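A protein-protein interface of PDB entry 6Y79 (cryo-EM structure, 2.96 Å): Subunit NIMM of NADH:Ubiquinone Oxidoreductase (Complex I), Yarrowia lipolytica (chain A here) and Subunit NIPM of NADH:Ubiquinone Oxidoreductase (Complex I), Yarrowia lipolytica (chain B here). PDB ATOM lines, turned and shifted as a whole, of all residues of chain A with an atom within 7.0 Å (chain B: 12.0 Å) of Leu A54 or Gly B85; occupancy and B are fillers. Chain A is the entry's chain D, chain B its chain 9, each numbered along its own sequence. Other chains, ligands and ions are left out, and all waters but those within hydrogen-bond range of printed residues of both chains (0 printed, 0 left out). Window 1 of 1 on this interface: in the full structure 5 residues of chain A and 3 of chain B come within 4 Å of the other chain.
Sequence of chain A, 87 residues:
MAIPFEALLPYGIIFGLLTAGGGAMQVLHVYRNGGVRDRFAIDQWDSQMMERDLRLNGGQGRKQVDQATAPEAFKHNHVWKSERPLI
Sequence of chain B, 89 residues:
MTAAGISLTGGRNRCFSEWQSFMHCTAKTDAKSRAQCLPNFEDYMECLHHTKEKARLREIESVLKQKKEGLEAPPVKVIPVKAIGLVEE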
ATOM      1  N   MET A  49      -5.059 -32.532  20.032  1.00  0.00           N
ATOM      2  CA  MET A  49      -4.887 -33.467  21.137  1.00  0.00           C
ATOM      3  C   MET A  49      -3.732 -33.056  22.046  1.00  0.00           C
ATOM      4  O   MET A  49      -3.820 -33.176  23.278  1.00  0.00           O
ATOM      5  CB  MET A  49      -4.679 -34.875  20.595  1.00  0.00           C
ATOM      6  CG  MET A  49      -4.867 -35.883  21.639  1.00  0.00           C
ATOM      7  SD  MET A  49      -6.493 -35.871  22.397  1.00  0.00           S
ATOM      8  CE  MET A  49      -7.374 -36.738  21.128  1.00  0.00           C
ATOM      9  N   MET A  50      -2.663 -32.509  21.459  1.00  0.00           N
ATOM     10  CA  MET A  50      -1.541 -32.000  22.239  1.00  0.00           C
ATOM     11  C   MET A  50      -1.930 -30.786  23.076  1.00  0.00           C
ATOM     12  O   MET A  50      -1.497 -30.667  24.225  1.00  0.00           O
ATOM     13  CB  MET A  50      -0.375 -31.652  21.321  1.00  0.00           C
ATOM     14  CG  MET A  50       0.384 -32.846  20.821  1.00  0.00           C
ATOM     15  SD  MET A  50       1.621 -32.377  19.609  1.00  0.00           S
ATOM     16  CE  MET A  50       2.909 -31.767  20.687  1.00  0.00           C
ATOM     17  N   GLU A  51      -2.723 -29.862  22.523  1.00  0.00           N
ATOM     18  CA  GLU A  51      -3.160 -28.728  23.343  1.00  0.00           C
ATOM     19  C   GLU A  51      -4.144 -29.167  24.426  1.00  0.00           C
ATOM     20  O   GLU A  51      -4.145 -28.601  25.528  1.00  0.00           O
ATOM     21  CB  GLU A  51      -3.743 -27.614  22.474  1.00  0.00           C
ATOM     22  CG  GLU A  51      -5.047 -27.980  21.858  1.00  0.00           C
ATOM     23  CD  GLU A  51      -5.569 -27.055  20.825  1.00  0.00           C
ATOM     24  OE1 GLU A  51      -4.963 -26.002  20.480  1.00  0.00           O
ATOM     25  OE2 GLU A  51      -6.619 -27.440  20.214  1.00  0.00           O
ATOM     26  N   ARG A  52      -4.925 -30.228  24.171  1.00  0.00           N
ATOM     27  CA  ARG A  52      -5.814 -30.733  25.215  1.00  0.00           C
ATOM     28  C   ARG A  52      -5.030 -31.375  26.354  1.00  0.00           C
ATOM     29  O   ARG A  52      -5.376 -31.227  27.533  1.00  0.00           O
ATOM     30  CB  ARG A  52      -6.798 -31.737  24.623  1.00  0.00           C
ATOM     31  CG  ARG A  52      -7.787 -32.256  25.610  1.00  0.00           C
ATOM     32  CD  ARG A  52      -8.690 -33.273  24.993  1.00  0.00           C
ATOM     33  NE  ARG A  52      -9.627 -33.777  25.984  1.00  0.00           N
ATOM     34  CZ  ARG A  52      -9.378 -34.802  26.787  1.00  0.00           C
ATOM     35  NH1 ARG A  52      -8.221 -35.442  26.715  1.00  0.00           N
ATOM     36  NH2 ARG A  52     -10.293 -35.186  27.658  1.00  0.00           N
ATOM     37  N   ASP A  53      -3.942 -32.057  26.025  1.00  0.00           N
ATOM     38  CA  ASP A  53      -3.165 -32.696  27.079  1.00  0.00           C
ATOM     39  C   ASP A  53      -2.308 -31.696  27.841  1.00  0.00           C
ATOM     40  O   ASP A  53      -2.055 -31.892  29.034  1.00  0.00           O
ATOM     41  CB  ASP A  53      -2.318 -33.810  26.500  1.00  0.00           C
ATOM     42  CG  ASP A  53      -3.152 -34.861  25.834  1.00  0.00           C
ATOM     43  OD1 ASP A  53      -4.398 -34.837  25.962  1.00  0.00           O
ATOM     44  OD2 ASP A  53      -2.549 -35.705  25.170  1.00  0.00           O
ATOM     45  N   LEU A  54      -1.869 -30.610  27.187  1.00  0.00           N
ATOM     46  CA  LEU A  54      -1.261 -29.511  27.936  1.00  0.00           C
ATOM     47  C   LEU A  54      -2.270 -28.866  28.872  1.00  0.00           C
ATOM     48  O   LEU A  54      -1.903 -28.407  29.958  1.00  0.00           O
ATOM     49  CB  LEU A  54      -0.678 -28.467  26.978  1.00  0.00           C
ATOM     50  CG  LEU A  54       0.174 -27.275  27.434  1.00  0.00           C
ATOM     51  CD1 LEU A  54       1.091 -26.887  26.295  1.00  0.00           C
ATOM     52  CD2 LEU A  54      -0.599 -26.040  27.870  1.00  0.00           C
ATOM     53  N   ARG A  55      -3.539 -28.823  28.469  1.00  0.00           N
ATOM     54  CA  ARG A  55      -4.574 -28.321  29.364  1.00  0.00           C
ATOM     55  C   ARG A  55      -4.818 -29.257  30.537  1.00  0.00           C
ATOM     56  O   ARG A  55      -5.088 -28.796  31.649  1.00  0.00           O
ATOM     57  CB  ARG A  55      -5.868 -28.113  28.577  1.00  0.00           C
ATOM     58  CG  ARG A  55      -6.959 -27.385  29.307  1.00  0.00           C
ATOM     59  CD  ARG A  55      -7.940 -26.800  28.326  1.00  0.00           C
ATOM     60  NE  ARG A  55      -8.357 -27.773  27.326  1.00  0.00           N
ATOM     61  CZ  ARG A  55      -9.488 -28.464  27.386  1.00  0.00           C
ATOM     62  NH1 ARG A  55     -10.314 -28.293  28.406  1.00  0.00           N
ATOM     63  NH2 ARG A  55      -9.792 -29.328  26.429  1.00  0.00           N
ATOM     64  N   LEU A  56      -4.709 -30.563  30.312  1.00  0.00           N
ATOM     65  CA  LEU A  56      -5.119 -31.518  31.333  1.00  0.00           C
ATOM     66  C   LEU A  56      -4.000 -31.813  32.326  1.00  0.00           C
ATOM     67  O   LEU A  56      -4.263 -32.003  33.516  1.00  0.00           O
ATOM     68  CB  LEU A  56      -5.608 -32.797  30.669  1.00  0.00           C
ATOM     69  CG  LEU A  56      -6.103 -33.960  31.513  1.00  0.00           C
ATOM     70  CD1 LEU A  56      -7.109 -33.533  32.562  1.00  0.00           C
ATOM     71  CD2 LEU A  56      -6.735 -34.908  30.539  1.00  0.00           C
ATOM     72  N   ASN A  57      -2.747 -31.889  31.862  1.00  0.00           N
ATOM     73  CA  ASN A  57      -1.678 -32.331  32.755  1.00  0.00           C
ATOM     74  C   ASN A  57      -1.302 -31.258  33.761  1.00  0.00           C
ATOM     75  O   ASN A  57      -0.939 -31.576  34.896  1.00  0.00           O
ATOM     76  CB  ASN A  57      -0.439 -32.797  31.967  1.00  0.00           C
ATOM     77  CG  ASN A  57       0.199 -31.704  31.101  1.00  0.00           C
ATOM     78  OD1 ASN A  57      -0.261 -30.567  31.030  1.00  0.00           O
ATOM     79  ND2 ASN A  57       1.272 -32.069  30.422  1.00  0.00           N
ATOM     80  N   GLY A  58      -1.415 -30.000  33.375  1.00  0.00           N
ATOM     81  CA  GLY A  58      -1.008 -28.915  34.225  1.00  0.00           C
ATOM     82  C   GLY A  58       0.352 -28.423  33.799  1.00  0.00           C
ATOM     83  O   GLY A  58       1.371 -28.982  34.213  1.00  0.00           O
ATOM     84  N   GLY A  59       0.391 -27.400  32.945  1.00  0.00           N
ATOM     85  CA  GLY A  59       1.632 -26.723  32.613  1.00  0.00           C
ATOM     86  C   GLY A  59       2.604 -27.461  31.713  1.00  0.00           C
ATOM     87  O   GLY A  59       3.082 -26.899  30.725  1.00  0.00           O
ATOM     88  N   GLN A  60       2.921 -28.705  32.068  1.00  0.00           N
ATOM     89  CA  GLN A  60       3.988 -29.461  31.430  1.00  0.00           C
ATOM     90  C   GLN A  60       3.609 -29.845  30.007  1.00  0.00           C
ATOM     91  O   GLN A  60       2.430 -29.925  29.658  1.00  0.00           O
ATOM     92  CB  GLN A  60       4.309 -30.717  32.240  1.00  0.00           C
ATOM     93  CG  GLN A  60       5.136 -30.472  33.502  1.00  0.00           C
ATOM     94  CD  GLN A  60       4.338 -29.832  34.625  1.00  0.00           C
ATOM     95  OE1 GLN A  60       4.674 -28.748  35.097  1.00  0.00           O
ATOM     96  NE2 GLN A  60       3.264 -30.493  35.040  1.00  0.00           N
ATOM     97  N   GLY A  61       4.629 -30.078  29.185  1.00  0.00           N
ATOM     98  CA  GLY A  61       4.438 -30.342  27.771  1.00  0.00           C
ATOM     99  C   GLY A  61       3.709 -31.630  27.454  1.00  0.00           C
ATOM    100  O   GLY A  61       2.566 -31.599  26.993  1.00  0.00           O
ATOM    101  N   ARG A  62       4.347 -32.768  27.703  1.00  0.00           N
ATOM    102  CA  ARG A  62       3.757 -34.078  27.447  1.00  0.00           C
ATOM    103  C   ARG A  62       3.990 -35.002  28.638  1.00  0.00           C
ATOM    104  O   ARG A  62       4.525 -36.105  28.514  1.00  0.00           O
ATOM    105  CB  ARG A  62       4.270 -34.664  26.133  1.00  0.00           C
ATOM    106  CG  ARG A  62       5.764 -34.586  25.897  1.00  0.00           C
ATOM    107  CD  ARG A  62       6.096 -35.150  24.526  1.00  0.00           C
ATOM    108  NE  ARG A  62       5.582 -36.506  24.371  1.00  0.00           N
ATOM    109  CZ  ARG A  62       5.706 -37.231  23.267  1.00  0.00           C
ATOM    110  NH1 ARG A  62       5.196 -38.448  23.214  1.00  0.00           N
ATOM    111  NH2 ARG A  62       6.355 -36.743  22.224  1.00  0.00           N
ATOM    112  N   GLN A  64       1.695 -36.438  30.414  1.00  0.00           N
ATOM    113  CA  GLN A  64       0.813 -37.566  30.119  1.00  0.00           C
ATOM    114  C   GLN A  64       0.323 -38.234  31.409  1.00  0.00           C
ATOM    115  O   GLN A  64       0.711 -39.335  31.803  1.00  0.00           O
ATOM    116  CB  GLN A  64       1.504 -38.537  29.163  1.00  0.00           C
ATOM    117  CG  GLN A  64       1.856 -37.921  27.824  1.00  0.00           C
ATOM    118  CD  GLN A  64       0.713 -37.974  26.866  1.00  0.00           C
ATOM    119  OE1 GLN A  64      -0.036 -38.931  26.892  1.00  0.00           O
ATOM    120  NE2 GLN A  64       0.587 -36.975  26.000  1.00  0.00           N
ATOM    121  N   ASN A  77     -10.253 -24.063  32.788  1.00  0.00           N
ATOM    122  CA  ASN A  77      -9.094 -23.553  32.069  1.00  0.00           C
ATOM    123  C   ASN A  77      -9.217 -23.724  30.560  1.00  0.00           C
ATOM    124  O   ASN A  77      -8.203 -23.691  29.858  1.00  0.00           O
ATOM    125  CB  ASN A  77      -7.798 -24.197  32.585  1.00  0.00           C
ATOM    126  CG  ASN A  77      -7.760 -25.711  32.425  1.00  0.00           C
ATOM    127  OD1 ASN A  77      -8.722 -26.341  31.997  1.00  0.00           O
ATOM    128  ND2 ASN A  77      -6.628 -26.301  32.782  1.00  0.00           N
ATOM    129  N   VAL A  79      -9.934 -23.040  26.608  1.00  0.00           N
ATOM    130  CA  VAL A  79      -9.495 -21.934  25.772  1.00  0.00           C
ATOM    131  C   VAL A  79     -10.325 -21.877  24.491  1.00  0.00           C
ATOM    132  O   VAL A  79     -10.626 -22.912  23.888  1.00  0.00           O
ATOM    133  CB  VAL A  79      -7.989 -22.110  25.488  1.00  0.00           C
ATOM    134  CG1 VAL A  79      -7.550 -21.392  24.243  1.00  0.00           C
ATOM    135  CG2 VAL A  79      -7.192 -21.654  26.680  1.00  0.00           C
ATOM    136  N   LYS B  77     -10.472 -13.989  30.957  1.00  0.00           N
ATOM    137  CA  LYS B  77      -9.029 -13.892  31.143  1.00  0.00           C
ATOM    138  C   LYS B  77      -8.351 -14.023  29.799  1.00  0.00           C
ATOM    139  O   LYS B  77      -8.868 -14.701  28.928  1.00  0.00           O
ATOM    140  CB  LYS B  77      -8.554 -14.988  32.066  1.00  0.00           C
ATOM    141  CG  LYS B  77      -7.066 -15.154  32.330  1.00  0.00           C
ATOM    142  CD  LYS B  77      -6.579 -14.244  33.459  1.00  0.00           C
ATOM    143  CE  LYS B  77      -5.236 -14.707  33.918  1.00  0.00           C
ATOM    144  NZ  LYS B  77      -4.383 -14.718  32.719  1.00  0.00           N
ATOM    145  N   VAL B  78      -7.251 -13.338  29.607  1.00  0.00           N
ATOM    146  CA  VAL B  78      -6.361 -13.631  28.485  1.00  0.00           C
ATOM    147  C   VAL B  78      -5.074 -14.242  29.018  1.00  0.00           C
ATOM    148  O   VAL B  78      -4.548 -13.804  30.046  1.00  0.00           O
ATOM    149  CB  VAL B  78      -6.108 -12.360  27.657  1.00  0.00           C
ATOM    150  CG1 VAL B  78      -4.949 -12.509  26.680  1.00  0.00           C
ATOM    151  CG2 VAL B  78      -7.359 -12.070  26.922  1.00  0.00           C
ATOM    152  N   ILE B  79      -4.600 -15.295  28.358  1.00  0.00           N
ATOM    153  CA  ILE B  79      -3.356 -15.952  28.740  1.00  0.00           C
ATOM    154  C   ILE B  79      -2.303 -15.766  27.657  1.00  0.00           C
ATOM    155  O   ILE B  79      -2.648 -15.482  26.501  1.00  0.00           O
ATOM    156  CB  ILE B  79      -3.599 -17.442  29.002  1.00  0.00           C
ATOM    157  CG1 ILE B  79      -4.437 -18.023  27.869  1.00  0.00           C
ATOM    158  CG2 ILE B  79      -4.246 -17.648  30.351  1.00  0.00           C
ATOM    159  CD1 ILE B  79      -4.628 -19.472  27.929  1.00  0.00           C
ATOM    160  N   PRO B  80      -1.023 -15.889  27.985  1.00  0.00           N
ATOM    161  CA  PRO B  80      -0.036 -16.195  26.953  1.00  0.00           C
ATOM    162  C   PRO B  80      -0.166 -17.648  26.530  1.00  0.00           C
ATOM    163  O   PRO B  80      -0.684 -18.495  27.260  1.00  0.00           O
ATOM    164  CB  PRO B  80       1.306 -15.938  27.645  1.00  0.00           C
ATOM    165  CG  PRO B  80       1.016 -16.145  29.092  1.00  0.00           C
ATOM    166  CD  PRO B  80      -0.395 -15.659  29.301  1.00  0.00           C
ATOM    167  N   VAL B  81       0.358 -17.931  25.334  1.00  0.00           N
ATOM    168  CA  VAL B  81       0.317 -19.282  24.777  1.00  0.00           C
ATOM    169  C   VAL B  81       1.220 -20.234  25.561  1.00  0.00           C
ATOM    170  O   VAL B  81       1.111 -21.459  25.432  1.00  0.00           O
ATOM    171  CB  VAL B  81       0.685 -19.228  23.281  1.00  0.00           C
ATOM    172  CG1 VAL B  81      -0.126 -18.145  22.587  1.00  0.00           C
ATOM    173  CG2 VAL B  81       2.165 -18.964  23.104  1.00  0.00           C
ATOM    174  N   LYS B  82       2.100 -19.691  26.397  1.00  0.00           N
ATOM    175  CA  LYS B  82       2.978 -20.444  27.274  1.00  0.00           C
ATOM    176  C   LYS B  82       2.241 -21.035  28.476  1.00  0.00           C
ATOM    177  O   LYS B  82       2.827 -21.835  29.209  1.00  0.00           O
ATOM    178  CB  LYS B  82       4.101 -19.531  27.754  1.00  0.00           C
ATOM    179  CG  LYS B  82       4.756 -18.716  26.648  1.00  0.00           C
ATOM    180  CD  LYS B  82       4.856 -17.233  27.028  1.00  0.00           C
ATOM    181  CE  LYS B  82       5.098 -16.394  25.772  1.00  0.00           C
ATOM    182  NZ  LYS B  82       4.593 -14.995  25.825  1.00  0.00           N
ATOM    183  N   ALA B  83       0.992 -20.636  28.719  1.00  0.00           N
ATOM    184  CA  ALA B  83       0.339 -20.816  30.016  1.00  0.00           C
ATOM    185  C   ALA B  83      -1.131 -21.202  29.863  1.00  0.00           C
ATOM    186  O   ALA B  83      -2.017 -20.604  30.480  1.00  0.00           O
ATOM    187  CB  ALA B  83       0.480 -19.548  30.836  1.00  0.00           C
ATOM    188  N   ILE B  84      -1.427 -22.194  29.018  1.00  0.00           N
ATOM    189  CA  ILE B  84      -2.822 -22.597  28.813  1.00  0.00           C
ATOM    190  C   ILE B  84      -3.327 -23.426  29.996  1.00  0.00           C
ATOM    191  O   ILE B  84      -4.452 -23.238  30.482  1.00  0.00           O
ATOM    192  CB  ILE B  84      -2.979 -23.329  27.463  1.00  0.00           C
ATOM    193  CG1 ILE B  84      -2.756 -22.319  26.335  1.00  0.00           C
ATOM    194  CG2 ILE B  84      -4.333 -24.037  27.317  1.00  0.00           C
ATOM    195  CD1 ILE B  84      -3.010 -22.836  24.948  1.00  0.00           C
ATOM    196  N   GLY B  85      -2.484 -24.312  30.515  1.00  0.00           N
ATOM    197  CA  GLY B  85      -2.896 -25.100  31.654  1.00  0.00           C
ATOM    198  C   GLY B  85      -2.030 -24.921  32.883  1.00  0.00           C
ATOM    199  O   GLY B  85      -1.731 -25.907  33.551  1.00  0.00           O
ATOM    200  N   LEU B  86      -1.643 -23.684  33.211  1.00  0.00           N
ATOM    201  CA  LEU B  86      -0.559 -23.454  34.169  1.00  0.00           C
ATOM    202  C   LEU B  86      -0.944 -23.860  35.591  1.00  0.00           C
ATOM    203  O   LEU B  86      -0.343 -24.772  36.168  1.00  0.00           O
ATOM    204  CB  LEU B  86      -0.130 -21.984  34.125  1.00  0.00           C
ATOM    205  CG  LEU B  86       1.094 -21.609  34.958  1.00  0.00           C
ATOM    206  CD1 LEU B  86       2.307 -22.427  34.543  1.00  0.00           C
ATOM    207  CD2 LEU B  86       1.385 -20.127  34.804  1.00  0.00           C
ATOM    208  N   VAL B  87      -1.947 -23.205  36.171  1.00  0.00           N
ATOM    209  CA  VAL B  87      -2.330 -23.530  37.537  1.00  0.00           C
ATOM    210  C   VAL B  87      -3.211 -24.772  37.549  1.00  0.00           C
ATOM    211  O   VAL B  87      -2.735 -25.876  37.807  1.00  0.00           O
ATOM    212  CB  VAL B  87      -3.043 -22.363  38.232  1.00  0.00           C
ATOM    213  CG1 VAL B  87      -4.268 -21.933  37.435  1.00  0.00           C
ATOM    214  CG2 VAL B  87      -3.429 -22.759  39.643  1.00  0.00           C
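The backbone carbonyl oxygen (O) of Gly B85 sits at hydrogen-bond distance from the backbone NH (N) of Gly A59 (2.7 Å).
The side-chain amide oxygen (OD1) of Asn A57 sits close to the backbone carbonyl oxygen (O) of Leu A54 (2.9 Å). O of Arg A55 is in hydrogen-bond range of ND2 of Asn A77, at 3.1 Å. The side-chain amide nitrogen of Gln A60 lies within hydrogen-bond range of the backbone carbonyl oxygen of Gly A58 (2.6 Å).
Among the printed residues, merely in contact across the chains: Leu A54 with Ile B84, Leu A54 with Gly B85, Gly A58 with Gly B85, Asn A77 with Ile B84, Val A79 with Ile B79 and Val A79 with Ile B84.
No residue of chain B comes within 4 Å of Leu A56. No residue of chain B comes within 4 Å of Asn A57. Of chain B, only Gly B85 (3.2 Å) comes within 4 Å of Gly A58. Gly A59 touches just one residue of chain B: Gly B85. Asn A77 touches just one residue of chain B: Ile B84 (3.8 Å). Of the printed residues of chain B, Val A79 touches Ile B79 and Ile B84. Printed residues of chain A within 4 Å of Ile B79: Val A79. Of the printed residues of chain A, Ile B84 touches Leu A54 (3.6 Å), Asn A77 (3.8 Å) and Val A79 (3.8 Å). Gly B85 touches just these residues of chain A: Leu A54 (3.7 Å), Gly A58 (3.2 Å) and Gly A59 (2.7 Å). The nearest residue of chain B that does not touch Leu A54 is Ala B83 (5.3 Å).
Of the 17 printed residues of chain A, 5 touch a printed residue of chain B. Among the printed residues, no Asp or Glu carboxylate lies within 4 Å of a Lys or Arg side-chain nitrogen of the other chain.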
